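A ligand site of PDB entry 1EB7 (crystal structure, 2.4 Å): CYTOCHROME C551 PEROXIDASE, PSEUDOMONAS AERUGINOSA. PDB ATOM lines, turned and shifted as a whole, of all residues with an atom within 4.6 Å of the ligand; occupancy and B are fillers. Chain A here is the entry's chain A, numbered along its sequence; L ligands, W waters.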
ATOM      1  N   PHE A  38     -13.603 -14.375  -7.177  1.00  0.00           N
ATOM      2  CA  PHE A  38     -13.131 -15.696  -6.862  1.00  0.00           C
ATOM      3  C   PHE A  38     -11.605 -15.811  -6.961  1.00  0.00           C
ATOM      4  O   PHE A  38     -10.990 -16.669  -6.312  1.00  0.00           O
ATOM      5  CB  PHE A  38     -13.795 -16.654  -7.842  1.00  0.00           C
ATOM      6  CG  PHE A  38     -13.530 -18.099  -7.558  1.00  0.00           C
ATOM      7  CD1 PHE A  38     -14.340 -18.799  -6.682  1.00  0.00           C
ATOM      8  CD2 PHE A  38     -12.496 -18.762  -8.198  1.00  0.00           C
ATOM      9  CE1 PHE A  38     -14.124 -20.174  -6.449  1.00  0.00           C
ATOM     10  CE2 PHE A  38     -12.272 -20.124  -7.972  1.00  0.00           C
ATOM     11  CZ  PHE A  38     -13.093 -20.828  -7.087  1.00  0.00           C
ATOM     12  N   LEU A  49      -4.342 -14.939  -0.365  1.00  0.00           N
ATOM     13  CA  LEU A  49      -5.289 -16.044  -0.506  1.00  0.00           C
ATOM     14  C   LEU A  49      -6.500 -15.648  -1.310  1.00  0.00           C
ATOM     15  O   LEU A  49      -7.054 -14.585  -1.087  1.00  0.00           O
ATOM     16  CB  LEU A  49      -5.789 -16.530   0.853  1.00  0.00           C
ATOM     17  CG  LEU A  49      -4.939 -17.457   1.731  1.00  0.00           C
ATOM     18  CD1 LEU A  49      -5.628 -17.657   3.059  1.00  0.00           C
ATOM     19  CD2 LEU A  49      -4.739 -18.793   1.061  1.00  0.00           C
ATOM     20  N   SER A  50      -6.892 -16.511  -2.240  1.00  0.00           N
ATOM     21  CA  SER A  50      -8.073 -16.304  -3.057  1.00  0.00           C
ATOM     22  C   SER A  50      -8.817 -17.618  -2.988  1.00  0.00           C
ATOM     23  O   SER A  50      -8.232 -18.637  -2.587  1.00  0.00           O
ATOM     24  CB  SER A  50      -7.692 -16.038  -4.509  1.00  0.00           C
ATOM     25  OG  SER A  50      -7.221 -17.213  -5.147  1.00  0.00           O
ATOM     26  N   CYS A  51     -10.075 -17.629  -3.373  1.00  0.00           N
ATOM     27  CA  CYS A  51     -10.814 -18.893  -3.345  1.00  0.00           C
ATOM     28  C   CYS A  51     -10.064 -19.906  -4.197  1.00  0.00           C
ATOM     29  O   CYS A  51      -9.930 -21.065  -3.816  1.00  0.00           O
ATOM     30  CB  CYS A  51     -12.188 -18.713  -3.958  1.00  0.00           C
ATOM     31  SG  CYS A  51     -13.188 -17.458  -3.151  1.00  0.00           S
ATOM     32  N   CYS A  54      -7.264 -22.510  -2.796  1.00  0.00           N
ATOM     33  CA  CYS A  54      -7.645 -23.804  -2.256  1.00  0.00           C
ATOM     34  C   CYS A  54      -8.637 -24.600  -3.097  1.00  0.00           C
ATOM     35  O   CYS A  54      -8.753 -25.818  -2.942  1.00  0.00           O
ATOM     36  CB  CYS A  54      -8.211 -23.645  -0.860  1.00  0.00           C
ATOM     37  SG  CYS A  54      -7.163 -22.676   0.254  1.00  0.00           S
ATOM     38  N   HIS A  55      -9.365 -23.916  -3.972  1.00  0.00           N
ATOM     39  CA  HIS A  55     -10.347 -24.604  -4.822  1.00  0.00           C
ATOM     40  C   HIS A  55      -9.875 -24.342  -6.247  1.00  0.00           C
ATOM     41  O   HIS A  55     -10.549 -23.709  -7.056  1.00  0.00           O
ATOM     42  CB  HIS A  55     -11.765 -24.042  -4.579  1.00  0.00           C
ATOM     43  CG  HIS A  55     -12.266 -24.204  -3.168  1.00  0.00           C
ATOM     44  ND1 HIS A  55     -12.615 -25.422  -2.601  1.00  0.00           N
ATOM     45  CD2 HIS A  55     -12.469 -23.277  -2.189  1.00  0.00           C
ATOM     46  CE1 HIS A  55     -13.010 -25.172  -1.327  1.00  0.00           C
ATOM     47  NE2 HIS A  55     -12.950 -23.890  -1.026  1.00  0.00           N
ATOM     48  N   SER A  68      -6.144 -28.076   4.699  1.00  0.00           N
ATOM     49  CA  SER A  68      -5.924 -26.652   4.692  1.00  0.00           C
ATOM     50  C   SER A  68      -6.971 -26.099   5.647  1.00  0.00           C
ATOM     51  O   SER A  68      -7.788 -26.863   6.163  1.00  0.00           O
ATOM     52  CB  SER A  68      -6.086 -26.070   3.290  1.00  0.00           C
ATOM     53  OG  SER A  68      -7.398 -26.239   2.851  1.00  0.00           O
ATOM     54  N   VAL A  69      -6.932 -24.810   5.938  1.00  0.00           N
ATOM     55  CA  VAL A  69      -7.901 -24.223   6.864  1.00  0.00           C
ATOM     56  C   VAL A  69      -8.396 -22.992   6.194  1.00  0.00           C
ATOM     57  O   VAL A  69      -7.706 -21.966   6.219  1.00  0.00           O
ATOM     58  CB  VAL A  69      -7.248 -23.795   8.181  1.00  0.00           C
ATOM     59  CG1 VAL A  69      -8.227 -22.954   9.002  1.00  0.00           C
ATOM     60  CG2 VAL A  69      -6.822 -25.011   8.971  1.00  0.00           C
ATOM     61  N   GLY A  70      -9.592 -23.049   5.622  1.00  0.00           N
ATOM     62  CA  GLY A  70     -10.089 -21.884   4.918  1.00  0.00           C
ATOM     63  C   GLY A  70     -11.371 -21.255   5.369  1.00  0.00           C
ATOM     64  O   GLY A  70     -11.648 -20.112   5.016  1.00  0.00           O
ATOM     65  N   HIS A  71     -12.158 -21.979   6.171  1.00  0.00           N
ATOM     66  CA  HIS A  71     -13.439 -21.467   6.640  1.00  0.00           C
ATOM     67  C   HIS A  71     -13.571 -21.533   8.159  1.00  0.00           C
ATOM     68  O   HIS A  71     -13.082 -22.470   8.804  1.00  0.00           O
ATOM     69  CB  HIS A  71     -14.582 -22.209   5.951  1.00  0.00           C
ATOM     70  CG  HIS A  71     -14.549 -22.077   4.457  1.00  0.00           C
ATOM     71  ND1 HIS A  71     -15.220 -21.105   3.734  1.00  0.00           N
ATOM     72  CD2 HIS A  71     -13.914 -22.831   3.524  1.00  0.00           C
ATOM     73  CE1 HIS A  71     -14.963 -21.320   2.436  1.00  0.00           C
ATOM     74  NE2 HIS A  71     -14.173 -22.357   2.257  1.00  0.00           N
ATOM     75  N   TRP A  73     -15.963 -22.280  10.171  1.00  0.00           N
ATOM     76  CA  TRP A  73     -16.684 -23.399  10.759  1.00  0.00           C
ATOM     77  C   TRP A  73     -15.699 -24.446  11.308  1.00  0.00           C
ATOM     78  O   TRP A  73     -15.915 -25.043  12.361  1.00  0.00           O
ATOM     79  CB  TRP A  73     -17.590 -24.045   9.708  1.00  0.00           C
ATOM     80  CG  TRP A  73     -18.048 -25.421  10.083  1.00  0.00           C
ATOM     81  CD1 TRP A  73     -17.492 -26.585   9.667  1.00  0.00           C
ATOM     82  CD2 TRP A  73     -19.110 -25.767  10.986  1.00  0.00           C
ATOM     83  NE1 TRP A  73     -18.125 -27.645  10.273  1.00  0.00           N
ATOM     84  CE2 TRP A  73     -19.119 -27.170  11.085  1.00  0.00           C
ATOM     85  CE3 TRP A  73     -20.039 -25.027  11.741  1.00  0.00           C
ATOM     86  CZ2 TRP A  73     -20.027 -27.861  11.903  1.00  0.00           C
ATOM     87  CZ3 TRP A  73     -20.947 -25.719  12.560  1.00  0.00           C
ATOM     88  CH2 TRP A  73     -20.933 -27.122  12.629  1.00  0.00           C
ATOM     89  N   GLN A  74     -14.607 -24.642  10.568  1.00  0.00           N
ATOM     90  CA  GLN A  74     -13.562 -25.605  10.892  1.00  0.00           C
ATOM     91  C   GLN A  74     -13.065 -25.624  12.305  1.00  0.00           C
ATOM     92  O   GLN A  74     -12.669 -24.623  12.865  1.00  0.00           O
ATOM     93  CB  GLN A  74     -12.366 -25.439   9.944  1.00  0.00           C
ATOM     94  CG  GLN A  74     -12.700 -25.741   8.492  1.00  0.00           C
ATOM     95  CD  GLN A  74     -11.567 -25.412   7.539  1.00  0.00           C
ATOM     96  OE1 GLN A  74     -11.647 -24.443   6.769  1.00  0.00           O
ATOM     97  NE2 GLN A  74     -10.503 -26.205   7.571  1.00  0.00           N
ATOM     98  N   ARG A  78      -8.958 -29.574   7.249  1.00  0.00           N
ATOM     99  CA  ARG A  78      -9.738 -30.560   6.520  1.00  0.00           C
ATOM    100  C   ARG A  78      -9.298 -30.530   5.069  1.00  0.00           C
ATOM    101  O   ARG A  78      -8.667 -29.563   4.639  1.00  0.00           O
ATOM    102  CB  ARG A  78     -11.226 -30.214   6.594  1.00  0.00           C
ATOM    103  CG  ARG A  78     -11.815 -30.144   7.992  1.00  0.00           C
ATOM    104  CD  ARG A  78     -11.985 -31.551   8.506  1.00  0.00           C
ATOM    105  NE  ARG A  78     -12.658 -31.607   9.801  1.00  0.00           N
ATOM    106  CZ  ARG A  78     -12.026 -31.594  10.966  1.00  0.00           C
ATOM    107  NH1 ARG A  78     -10.708 -31.531  11.007  1.00  0.00           N
ATOM    108  NH2 ARG A  78     -12.733 -31.637  12.087  1.00  0.00           N
ATOM    109  N   ASN A  79      -9.623 -31.565   4.314  1.00  0.00           N
ATOM    110  CA  ASN A  79      -9.267 -31.604   2.915  1.00  0.00           C
ATOM    111  C   ASN A  79     -10.223 -30.657   2.206  1.00  0.00           C
ATOM    112  O   ASN A  79     -11.417 -30.667   2.500  1.00  0.00           O
ATOM    113  CB  ASN A  79      -9.447 -33.017   2.375  1.00  0.00           C
ATOM    114  CG  ASN A  79      -8.900 -33.192   0.985  1.00  0.00           C
ATOM    115  OD1 ASN A  79      -9.632 -33.532   0.016  1.00  0.00           O
ATOM    116  ND2 ASN A  79      -7.593 -32.976   0.851  1.00  0.00           N
ATOM    117  N   SER A  80      -9.704 -29.796   1.339  1.00  0.00           N
ATOM    118  CA  SER A  80     -10.569 -28.875   0.601  1.00  0.00           C
ATOM    119  C   SER A  80     -11.393 -29.632  -0.424  1.00  0.00           C
ATOM    120  O   SER A  80     -10.848 -30.333  -1.303  1.00  0.00           O
ATOM    121  CB  SER A  80      -9.738 -27.849  -0.149  1.00  0.00           C
ATOM    122  OG  SER A  80      -8.816 -27.230   0.724  1.00  0.00           O
ATOM    123  N   PRO A  81     -12.728 -29.548  -0.316  1.00  0.00           N
ATOM    124  CA  PRO A  81     -13.621 -30.223  -1.249  1.00  0.00           C
ATOM    125  C   PRO A  81     -13.651 -29.402  -2.534  1.00  0.00           C
ATOM    126  O   PRO A  81     -13.371 -28.191  -2.495  1.00  0.00           O
ATOM    127  CB  PRO A  81     -14.966 -30.131  -0.539  1.00  0.00           C
ATOM    128  CG  PRO A  81     -14.878 -28.778   0.105  1.00  0.00           C
ATOM    129  CD  PRO A  81     -13.493 -28.808   0.706  1.00  0.00           C
ATOM    130  N   THR A  82     -13.974 -30.039  -3.661  1.00  0.00           N
ATOM    131  CA  THR A  82     -14.018 -29.320  -4.916  1.00  0.00           C
ATOM    132  C   THR A  82     -15.144 -28.311  -4.890  1.00  0.00           C
ATOM    133  O   THR A  82     -16.125 -28.492  -4.173  1.00  0.00           O
ATOM    134  CB  THR A  82     -14.272 -30.253  -6.104  1.00  0.00           C
ATOM    135  OG1 THR A  82     -14.452 -29.464  -7.284  1.00  0.00           O
ATOM    136  CG2 THR A  82     -15.503 -31.091  -5.880  1.00  0.00           C
ATOM    137  N   VAL A  83     -15.031 -27.264  -5.682  1.00  0.00           N
ATOM    138  CA  VAL A  83     -16.069 -26.258  -5.702  1.00  0.00           C
ATOM    139  C   VAL A  83     -17.011 -26.559  -6.873  1.00  0.00           C
ATOM    140  O   VAL A  83     -18.087 -25.960  -6.994  1.00  0.00           O
ATOM    141  CB  VAL A  83     -15.469 -24.847  -5.855  1.00  0.00           C
ATOM    142  CG1 VAL A  83     -14.881 -24.669  -7.246  1.00  0.00           C
ATOM    143  CG2 VAL A  83     -16.518 -23.801  -5.582  1.00  0.00           C
ATOM    144  N   ALA A  86     -20.770 -27.602  -6.371  1.00  0.00           N
ATOM    145  CA  ALA A  86     -21.082 -27.430  -4.963  1.00  0.00           C
ATOM    146  C   ALA A  86     -22.425 -26.773  -4.747  1.00  0.00           C
ATOM    147  O   ALA A  86     -23.083 -26.995  -3.737  1.00  0.00           O
ATOM    148  CB  ALA A  86     -20.001 -26.640  -4.269  1.00  0.00           C
ATOM    149  N   ASN A  89     -25.237 -28.884  -3.335  1.00  0.00           N
ATOM    150  CA  ASN A  89     -25.109 -29.577  -2.059  1.00  0.00           C
ATOM    151  C   ASN A  89     -25.891 -28.894  -0.967  1.00  0.00           C
ATOM    152  O   ASN A  89     -25.755 -27.700  -0.718  1.00  0.00           O
ATOM    153  CB  ASN A  89     -23.643 -29.638  -1.652  1.00  0.00           C
ATOM    154  CG  ASN A  89     -22.830 -30.521  -2.566  1.00  0.00           C
ATOM    155  OD1 ASN A  89     -23.334 -31.493  -3.138  1.00  0.00           O
ATOM    156  ND2 ASN A  89     -21.568 -30.164  -2.737  1.00  0.00           N
ATOM    157  N   ALA A  91     -25.839 -30.129   2.190  1.00  0.00           N
ATOM    158  CA  ALA A  91     -24.916 -30.250   3.310  1.00  0.00           C
ATOM    159  C   ALA A  91     -23.566 -29.730   2.798  1.00  0.00           C
ATOM    160  O   ALA A  91     -22.986 -30.281   1.880  1.00  0.00           O
ATOM    161  CB  ALA A  91     -24.796 -31.708   3.714  1.00  0.00           C
ATOM    162  N   GLN A  92     -23.055 -28.672   3.418  1.00  0.00           N
ATOM    163  CA  GLN A  92     -21.817 -28.079   2.943  1.00  0.00           C
ATOM    164  C   GLN A  92     -20.510 -28.458   3.594  1.00  0.00           C
ATOM    165  O   GLN A  92     -19.523 -28.665   2.905  1.00  0.00           O
ATOM    166  CB  GLN A  92     -21.964 -26.573   2.944  1.00  0.00           C
ATOM    167  CG  GLN A  92     -23.140 -26.148   2.139  1.00  0.00           C
ATOM    168  CD  GLN A  92     -23.502 -24.720   2.364  1.00  0.00           C
ATOM    169  OE1 GLN A  92     -23.607 -24.257   3.507  1.00  0.00           O
ATOM    170  NE2 GLN A  92     -23.692 -23.981   1.276  1.00  0.00           N
ATOM    171  N   PHE A  93     -20.469 -28.554   4.916  1.00  0.00           N
ATOM    172  CA  PHE A  93     -19.208 -28.862   5.577  1.00  0.00           C
ATOM    173  C   PHE A  93     -18.985 -30.323   5.896  1.00  0.00           C
ATOM    174  O   PHE A  93     -19.933 -31.112   5.907  1.00  0.00           O
ATOM    175  CB  PHE A  93     -19.071 -27.972   6.799  1.00  0.00           C
ATOM    176  CG  PHE A  93     -19.243 -26.522   6.492  1.00  0.00           C
ATOM    177  CD1 PHE A  93     -20.342 -25.807   6.984  1.00  0.00           C
ATOM    178  CD2 PHE A  93     -18.321 -25.850   5.681  1.00  0.00           C
ATOM    179  CE1 PHE A  93     -20.523 -24.451   6.668  1.00  0.00           C
ATOM    180  CE2 PHE A  93     -18.493 -24.492   5.366  1.00  0.00           C
ATOM    181  CZ  PHE A  93     -19.587 -23.796   5.854  1.00  0.00           C
ATOM    182  N   TRP A  94     -17.732 -30.669   6.171  1.00  0.00           N
ATOM    183  CA  TRP A  94     -17.351 -32.038   6.469  1.00  0.00           C
ATOM    184  C   TRP A  94     -17.985 -32.684   7.675  1.00  0.00           C
ATOM    185  O   TRP A  94     -18.543 -33.762   7.588  1.00  0.00           O
ATOM    186  CB  TRP A  94     -15.843 -32.139   6.677  1.00  0.00           C
ATOM    187  CG  TRP A  94     -15.055 -32.276   5.446  1.00  0.00           C
ATOM    188  CD1 TRP A  94     -14.165 -31.371   4.932  1.00  0.00           C
ATOM    189  CD2 TRP A  94     -15.036 -33.420   4.574  1.00  0.00           C
ATOM    190  NE1 TRP A  94     -13.587 -31.884   3.795  1.00  0.00           N
ATOM    191  CE2 TRP A  94     -14.095 -33.122   3.550  1.00  0.00           C
ATOM    192  CE3 TRP A  94     -15.707 -34.640   4.555  1.00  0.00           C
ATOM    193  CZ2 TRP A  94     -13.810 -34.024   2.531  1.00  0.00           C
ATOM    194  CZ3 TRP A  94     -15.423 -35.542   3.536  1.00  0.00           C
ATOM    195  CH2 TRP A  94     -14.487 -35.228   2.534  1.00  0.00           C
ATOM    196  N   PRO A 108     -20.261 -20.971   3.271  1.00  0.00           N
ATOM    197  CA  PRO A 108     -18.831 -20.998   2.957  1.00  0.00           C
ATOM    198  C   PRO A 108     -18.219 -19.641   2.712  1.00  0.00           C
ATOM    199  O   PRO A 108     -17.112 -19.347   3.180  1.00  0.00           O
ATOM    200  CB  PRO A 108     -18.780 -21.813   1.671  1.00  0.00           C
ATOM    201  CG  PRO A 108     -19.924 -22.720   1.807  1.00  0.00           C
ATOM    202  CD  PRO A 108     -21.005 -21.806   2.318  1.00  0.00           C
ATOM    203  N   ILE A 109     -18.940 -18.787   2.004  1.00  0.00           N
ATOM    204  CA  ILE A 109     -18.420 -17.487   1.670  1.00  0.00           C
ATOM    205  C   ILE A 109     -18.245 -16.563   2.861  1.00  0.00           C
ATOM    206  O   ILE A 109     -17.161 -16.010   3.071  1.00  0.00           O
ATOM    207  CB  ILE A 109     -19.277 -16.846   0.573  1.00  0.00           C
ATOM    208  CG1 ILE A 109     -19.285 -17.770  -0.636  1.00  0.00           C
ATOM    209  CG2 ILE A 109     -18.746 -15.473   0.193  1.00  0.00           C
ATOM    210  CD1 ILE A 109     -20.144 -17.300  -1.766  1.00  0.00           C
ATOM    211  N   SER A 112     -15.416 -17.901   5.211  1.00  0.00           N
ATOM    212  CA  SER A 112     -14.070 -17.678   4.724  1.00  0.00           C
ATOM    213  C   SER A 112     -13.642 -16.218   4.904  1.00  0.00           C
ATOM    214  O   SER A 112     -12.563 -15.920   5.432  1.00  0.00           O
ATOM    215  CB  SER A 112     -14.021 -18.074   3.243  1.00  0.00           C
ATOM    216  OG  SER A 112     -12.746 -17.852   2.669  1.00  0.00           O
ATOM    217  N   HIS A 116     -10.350 -15.017   7.072  1.00  0.00           N
ATOM    218  CA  HIS A 116      -9.146 -14.406   6.506  1.00  0.00           C
ATOM    219  C   HIS A 116      -9.185 -12.906   6.382  1.00  0.00           C
ATOM    220  O   HIS A 116      -8.240 -12.287   5.909  1.00  0.00           O
ATOM    221  CB  HIS A 116      -8.836 -15.048   5.161  1.00  0.00           C
ATOM    222  CG  HIS A 116      -8.684 -16.538   5.254  1.00  0.00           C
ATOM    223  ND1 HIS A 116      -7.650 -17.150   5.931  1.00  0.00           N
ATOM    224  CD2 HIS A 116      -9.459 -17.548   4.787  1.00  0.00           C
ATOM    225  CE1 HIS A 116      -7.804 -18.466   5.882  1.00  0.00           C
ATOM    226  NE2 HIS A 116      -8.893 -18.729   5.196  1.00  0.00           N
ATOM    227  N   ILE A 156     -20.282 -14.114  -6.149  1.00  0.00           N
ATOM    228  CA  ILE A 156     -19.494 -15.331  -6.076  1.00  0.00           C
ATOM    229  C   ILE A 156     -20.357 -16.561  -6.286  1.00  0.00           C
ATOM    230  O   ILE A 156     -19.942 -17.493  -6.964  1.00  0.00           O
ATOM    231  CB  ILE A 156     -18.707 -15.415  -4.745  1.00  0.00           C
ATOM    232  CG1 ILE A 156     -17.600 -14.352  -4.753  1.00  0.00           C
ATOM    233  CG2 ILE A 156     -18.103 -16.811  -4.548  1.00  0.00           C
ATOM    234  CD1 ILE A 156     -16.777 -14.271  -3.490  1.00  0.00           C
ATOM    235  N   GLU A 160     -20.040 -19.424  -8.965  1.00  0.00           N
ATOM    236  CA  GLU A 160     -20.050 -20.811  -8.537  1.00  0.00           C
ATOM    237  C   GLU A 160     -21.024 -21.647  -9.365  1.00  0.00           C
ATOM    238  O   GLU A 160     -20.728 -22.790  -9.704  1.00  0.00           O
ATOM    239  CB  GLU A 160     -20.434 -20.925  -7.067  1.00  0.00           C
ATOM    240  CG  GLU A 160     -19.347 -20.434  -6.144  1.00  0.00           C
ATOM    241  CD  GLU A 160     -19.518 -20.945  -4.744  1.00  0.00           C
ATOM    242  OE1 GLU A 160     -19.128 -22.090  -4.474  1.00  0.00           O
ATOM    243  OE2 GLU A 160     -20.055 -20.216  -3.900  1.00  0.00           O
ATOM    244  N   ARG A 246     -20.336 -35.481   6.703  1.00  0.00           N
ATOM    245  CA  ARG A 246     -21.122 -35.377   5.498  1.00  0.00           C
ATOM    246  C   ARG A 246     -20.732 -36.472   4.532  1.00  0.00           C
ATOM    247  O   ARG A 246     -19.583 -36.879   4.481  1.00  0.00           O
ATOM    248  CB  ARG A 246     -20.829 -34.021   4.903  1.00  0.00           C
ATOM    249  CG  ARG A 246     -21.327 -33.769   3.524  1.00  0.00           C
ATOM    250  CD  ARG A 246     -20.179 -33.105   2.820  1.00  0.00           C
ATOM    251  NE  ARG A 246     -20.600 -32.057   1.927  1.00  0.00           N
ATOM    252  CZ  ARG A 246     -19.836 -31.542   0.981  1.00  0.00           C
ATOM    253  NH1 ARG A 246     -18.598 -31.972   0.821  1.00  0.00           N
ATOM    254  NH2 ARG A 246     -20.310 -30.598   0.197  1.00  0.00           N
HETATM  255 FE1  LIG L   1     -13.501 -23.094   0.616  1.00  0.00          FE
HETATM  256  C1  LIG L   1     -15.198 -25.713   1.740  1.00  0.00           C
HETATM  257  C2  LIG L   1     -15.936 -22.201  -1.412  1.00  0.00           C
HETATM  258  C3  LIG L   1     -12.046 -20.065   0.226  1.00  0.00           C
HETATM  259  C4  LIG L   1     -10.686 -24.228   2.014  1.00  0.00           C
HETATM  260  N1  LIG L   1     -15.233 -23.734   0.299  1.00  0.00           N
HETATM  261  C5  LIG L   1     -15.852 -24.811   0.903  1.00  0.00           C
HETATM  262  C6  LIG L   1     -17.185 -25.019   0.362  1.00  0.00           C
HETATM  263  C7  LIG L   1     -17.337 -24.100  -0.576  1.00  0.00           C
HETATM  264  C8  LIG L   1     -16.141 -23.301  -0.617  1.00  0.00           C
HETATM  265  C9  LIG L   1     -18.456 -24.112  -1.543  1.00  0.00           C
HETATM  266  C10 LIG L   1     -18.242 -26.069   0.713  1.00  0.00           C
HETATM  267  C11 LIG L   1     -18.193 -27.234  -0.293  1.00  0.00           C
HETATM  268  C12 LIG L   1     -19.569 -27.771  -0.675  1.00  0.00           C
HETATM  269  O1  LIG L   1     -19.635 -28.754  -1.450  1.00  0.00           O
HETATM  270  O2  LIG L   1     -20.592 -27.182  -0.253  1.00  0.00           O
HETATM  271  N2  LIG L   1     -13.894 -21.499  -0.334  1.00  0.00           N
HETATM  272  C13 LIG L   1     -14.896 -21.307  -1.252  1.00  0.00           C
HETATM  273  C14 LIG L   1     -14.957 -19.932  -1.759  1.00  0.00           C
HETATM  274  C15 LIG L   1     -13.921 -19.299  -1.181  1.00  0.00           C
HETATM  275  C16 LIG L   1     -13.289 -20.278  -0.288  1.00  0.00           C
HETATM  276  C17 LIG L   1     -16.023 -19.304  -2.630  1.00  0.00           C
HETATM  277  C18 LIG L   1     -13.447 -17.882  -1.414  1.00  0.00           C
HETATM  278  C19 LIG L   1     -14.424 -16.773  -0.990  1.00  0.00           C
HETATM  279  N3  LIG L   1     -11.734 -22.382   0.857  1.00  0.00           N
HETATM  280  C20 LIG L   1     -11.272 -21.119   0.655  1.00  0.00           C
HETATM  281  C21 LIG L   1      -9.856 -20.988   0.973  1.00  0.00           C
HETATM  282  C22 LIG L   1      -9.466 -22.207   1.372  1.00  0.00           C
HETATM  283  C23 LIG L   1     -10.643 -23.023   1.360  1.00  0.00           C
HETATM  284  C24 LIG L   1      -9.046 -19.702   0.914  1.00  0.00           C
HETATM  285  C25 LIG L   1      -8.088 -22.679   1.755  1.00  0.00           C
HETATM  286  C26 LIG L   1      -7.339 -21.872   2.814  1.00  0.00           C
HETATM  287  N4  LIG L   1     -13.053 -24.634   1.621  1.00  0.00           N
HETATM  288  C27 LIG L   1     -11.835 -24.960   2.153  1.00  0.00           C
HETATM  289  C28 LIG L   1     -11.884 -26.134   2.976  1.00  0.00           C
HETATM  290  C29 LIG L   1     -13.167 -26.539   2.973  1.00  0.00           C
HETATM  291  C30 LIG L   1     -13.867 -25.624   2.064  1.00  0.00           C
HETATM  292  C31 LIG L   1     -10.742 -26.767   3.739  1.00  0.00           C
HETATM  293  C32 LIG L   1     -13.774 -27.594   3.878  1.00  0.00           C
HETATM  294  C33 LIG L   1     -14.200 -26.974   5.200  1.00  0.00           C
HETATM  295  C34 LIG L   1     -15.029 -27.911   6.039  1.00  0.00           C
HETATM  296  O3  LIG L   1     -14.717 -28.100   7.232  1.00  0.00           O
HETATM  297  O4  LIG L   1     -16.015 -28.457   5.501  1.00  0.00           O
HETATM  298  O   HOH W   1     -16.784 -29.345   3.087  1.00  0.00           O
HETATM  299  O   HOH W   2     -17.987 -30.147  -3.071  1.00  0.00           O
HETATM  300  O   HOH W   3     -22.661 -25.330  -1.221  1.00  0.00           O
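The side-chain sulfur of Cys 54 is bonded to a carbon (C25) of the ligand, 1.8 Å away.
SG of Cys 51 is covalently linked to C18 of the ligand.
An iron atom (FE1) of the ligand is bound by a ring nitrogen (NE2) of His 55 (1.9 Å).
NE2 of His 71 is bound to FE1 of the ligand (1.9 Å).
NH2 of Arg 246 is in salt-bridge range of O1 of the ligand (2.6 Å).
The side-chain amide nitrogen (ND2) of Asn 89 lies within hydrogen-bond range of an oxygen (O1) of the ligand (2.7 Å).
The backbone NH (N) of Trp 94 is in hydrogen-bond range of an oxygen (O4) of the ligand (2.9 Å).
Water W1 lies within hydrogen-bond range of O4 of the ligand (2.7 Å), O of Gln 92 (2.8 Å) and N of Trp 94 (3.5 Å).
Water W2 lies within hydrogen-bond range of an oxygen (O1) of the ligand (2.7 Å) and the backbone carbonyl oxygen (O) of Thr 82 (2.7 Å).
Water W3 lies within hydrogen-bond range of an oxygen (O2) of the ligand, the side-chain amide nitrogen of Gln 92 and the backbone carbonyl oxygen of Ala 86.
Ser 50 touches the ligand (O to C24, 3.7 Å).
OG of Ser 68 touches C31 of the ligand, 3.5 Å away.
Val 69 touches the ligand.
CA of Gly 70 touches C26 of the ligand (3.5 Å).
CD1 of Trp 73 touches O3 of the ligand, at 3.99 Å.
CG of Gln 74 touches O3 of the ligand (3.3 Å).
O of Arg 78 touches C31 of the ligand, at 3.6 Å.
OG of Ser 80 touches C31 of the ligand, at 3.6 Å.
CD of Pro 81 touches C29 of the ligand, 3.2 Å away.
CB of Ala 86 touches O1 of the ligand (3.5 Å).
CB of Gln 92 touches O2 of the ligand, at 3.5 Å.
Phe 93 touches the ligand (CA to O4, 3.2 Å).
Pro 108 touches the ligand (CB to C7, 3.5 Å).
Ser 112 touches the ligand.
Ile 156 touches the ligand.
Glu 160 touches the ligand (OE1 to C9, 3.6 Å).
23 residues have an atom within 4 Å of the ligand: Ser 50, Cys 51, Cys 54, His 55, Ser 68, Val 69, Gly 70, His 71, Trp 73, Gln 74, Arg 78, Ser 80, Pro 81, Ala 86, Asn 89, Gln 92, Phe 93, Trp 94, Pro 108, Ser 112, Ile 156, Glu 160 and Arg 246.
Along chain A the residues within 4 Å of the ligand span positions 50 to 246.
The backbone NH of Cys 51 is in hydrogen-bond range of the backbone carbonyl oxygen of Phe 38, 3.2 Å away.
The backbone NH (N) of His 71 is in hydrogen-bond range of the side-chain amide oxygen (OE1) of Gln 74.
The backbone carbonyl oxygen of Trp 94 is in hydrogen-bond range of the backbone NH of Arg 246 (2.6 Å).
NH2 of Arg 246 lies within hydrogen-bond range of O of Gln 92, at 3.4 Å.
The side-chain amide oxygen of Gln 74 lies within hydrogen-bond range of the backbone NH of Gly 70 (2.7 Å).
The side-chain amide nitrogen (NE2) of Gln 74 sits at hydrogen-bond distance from the backbone carbonyl oxygen (O) of Ser 68, at 3.1 Å.
The backbone carbonyl oxygen (O) of Gly 70 is in hydrogen-bond range of the side-chain hydroxyl (OG) of Ser 112, at 3.4 Å.
O of Arg 78 is in hydrogen-bond range of N of Ser 68, 2.9 Å away.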
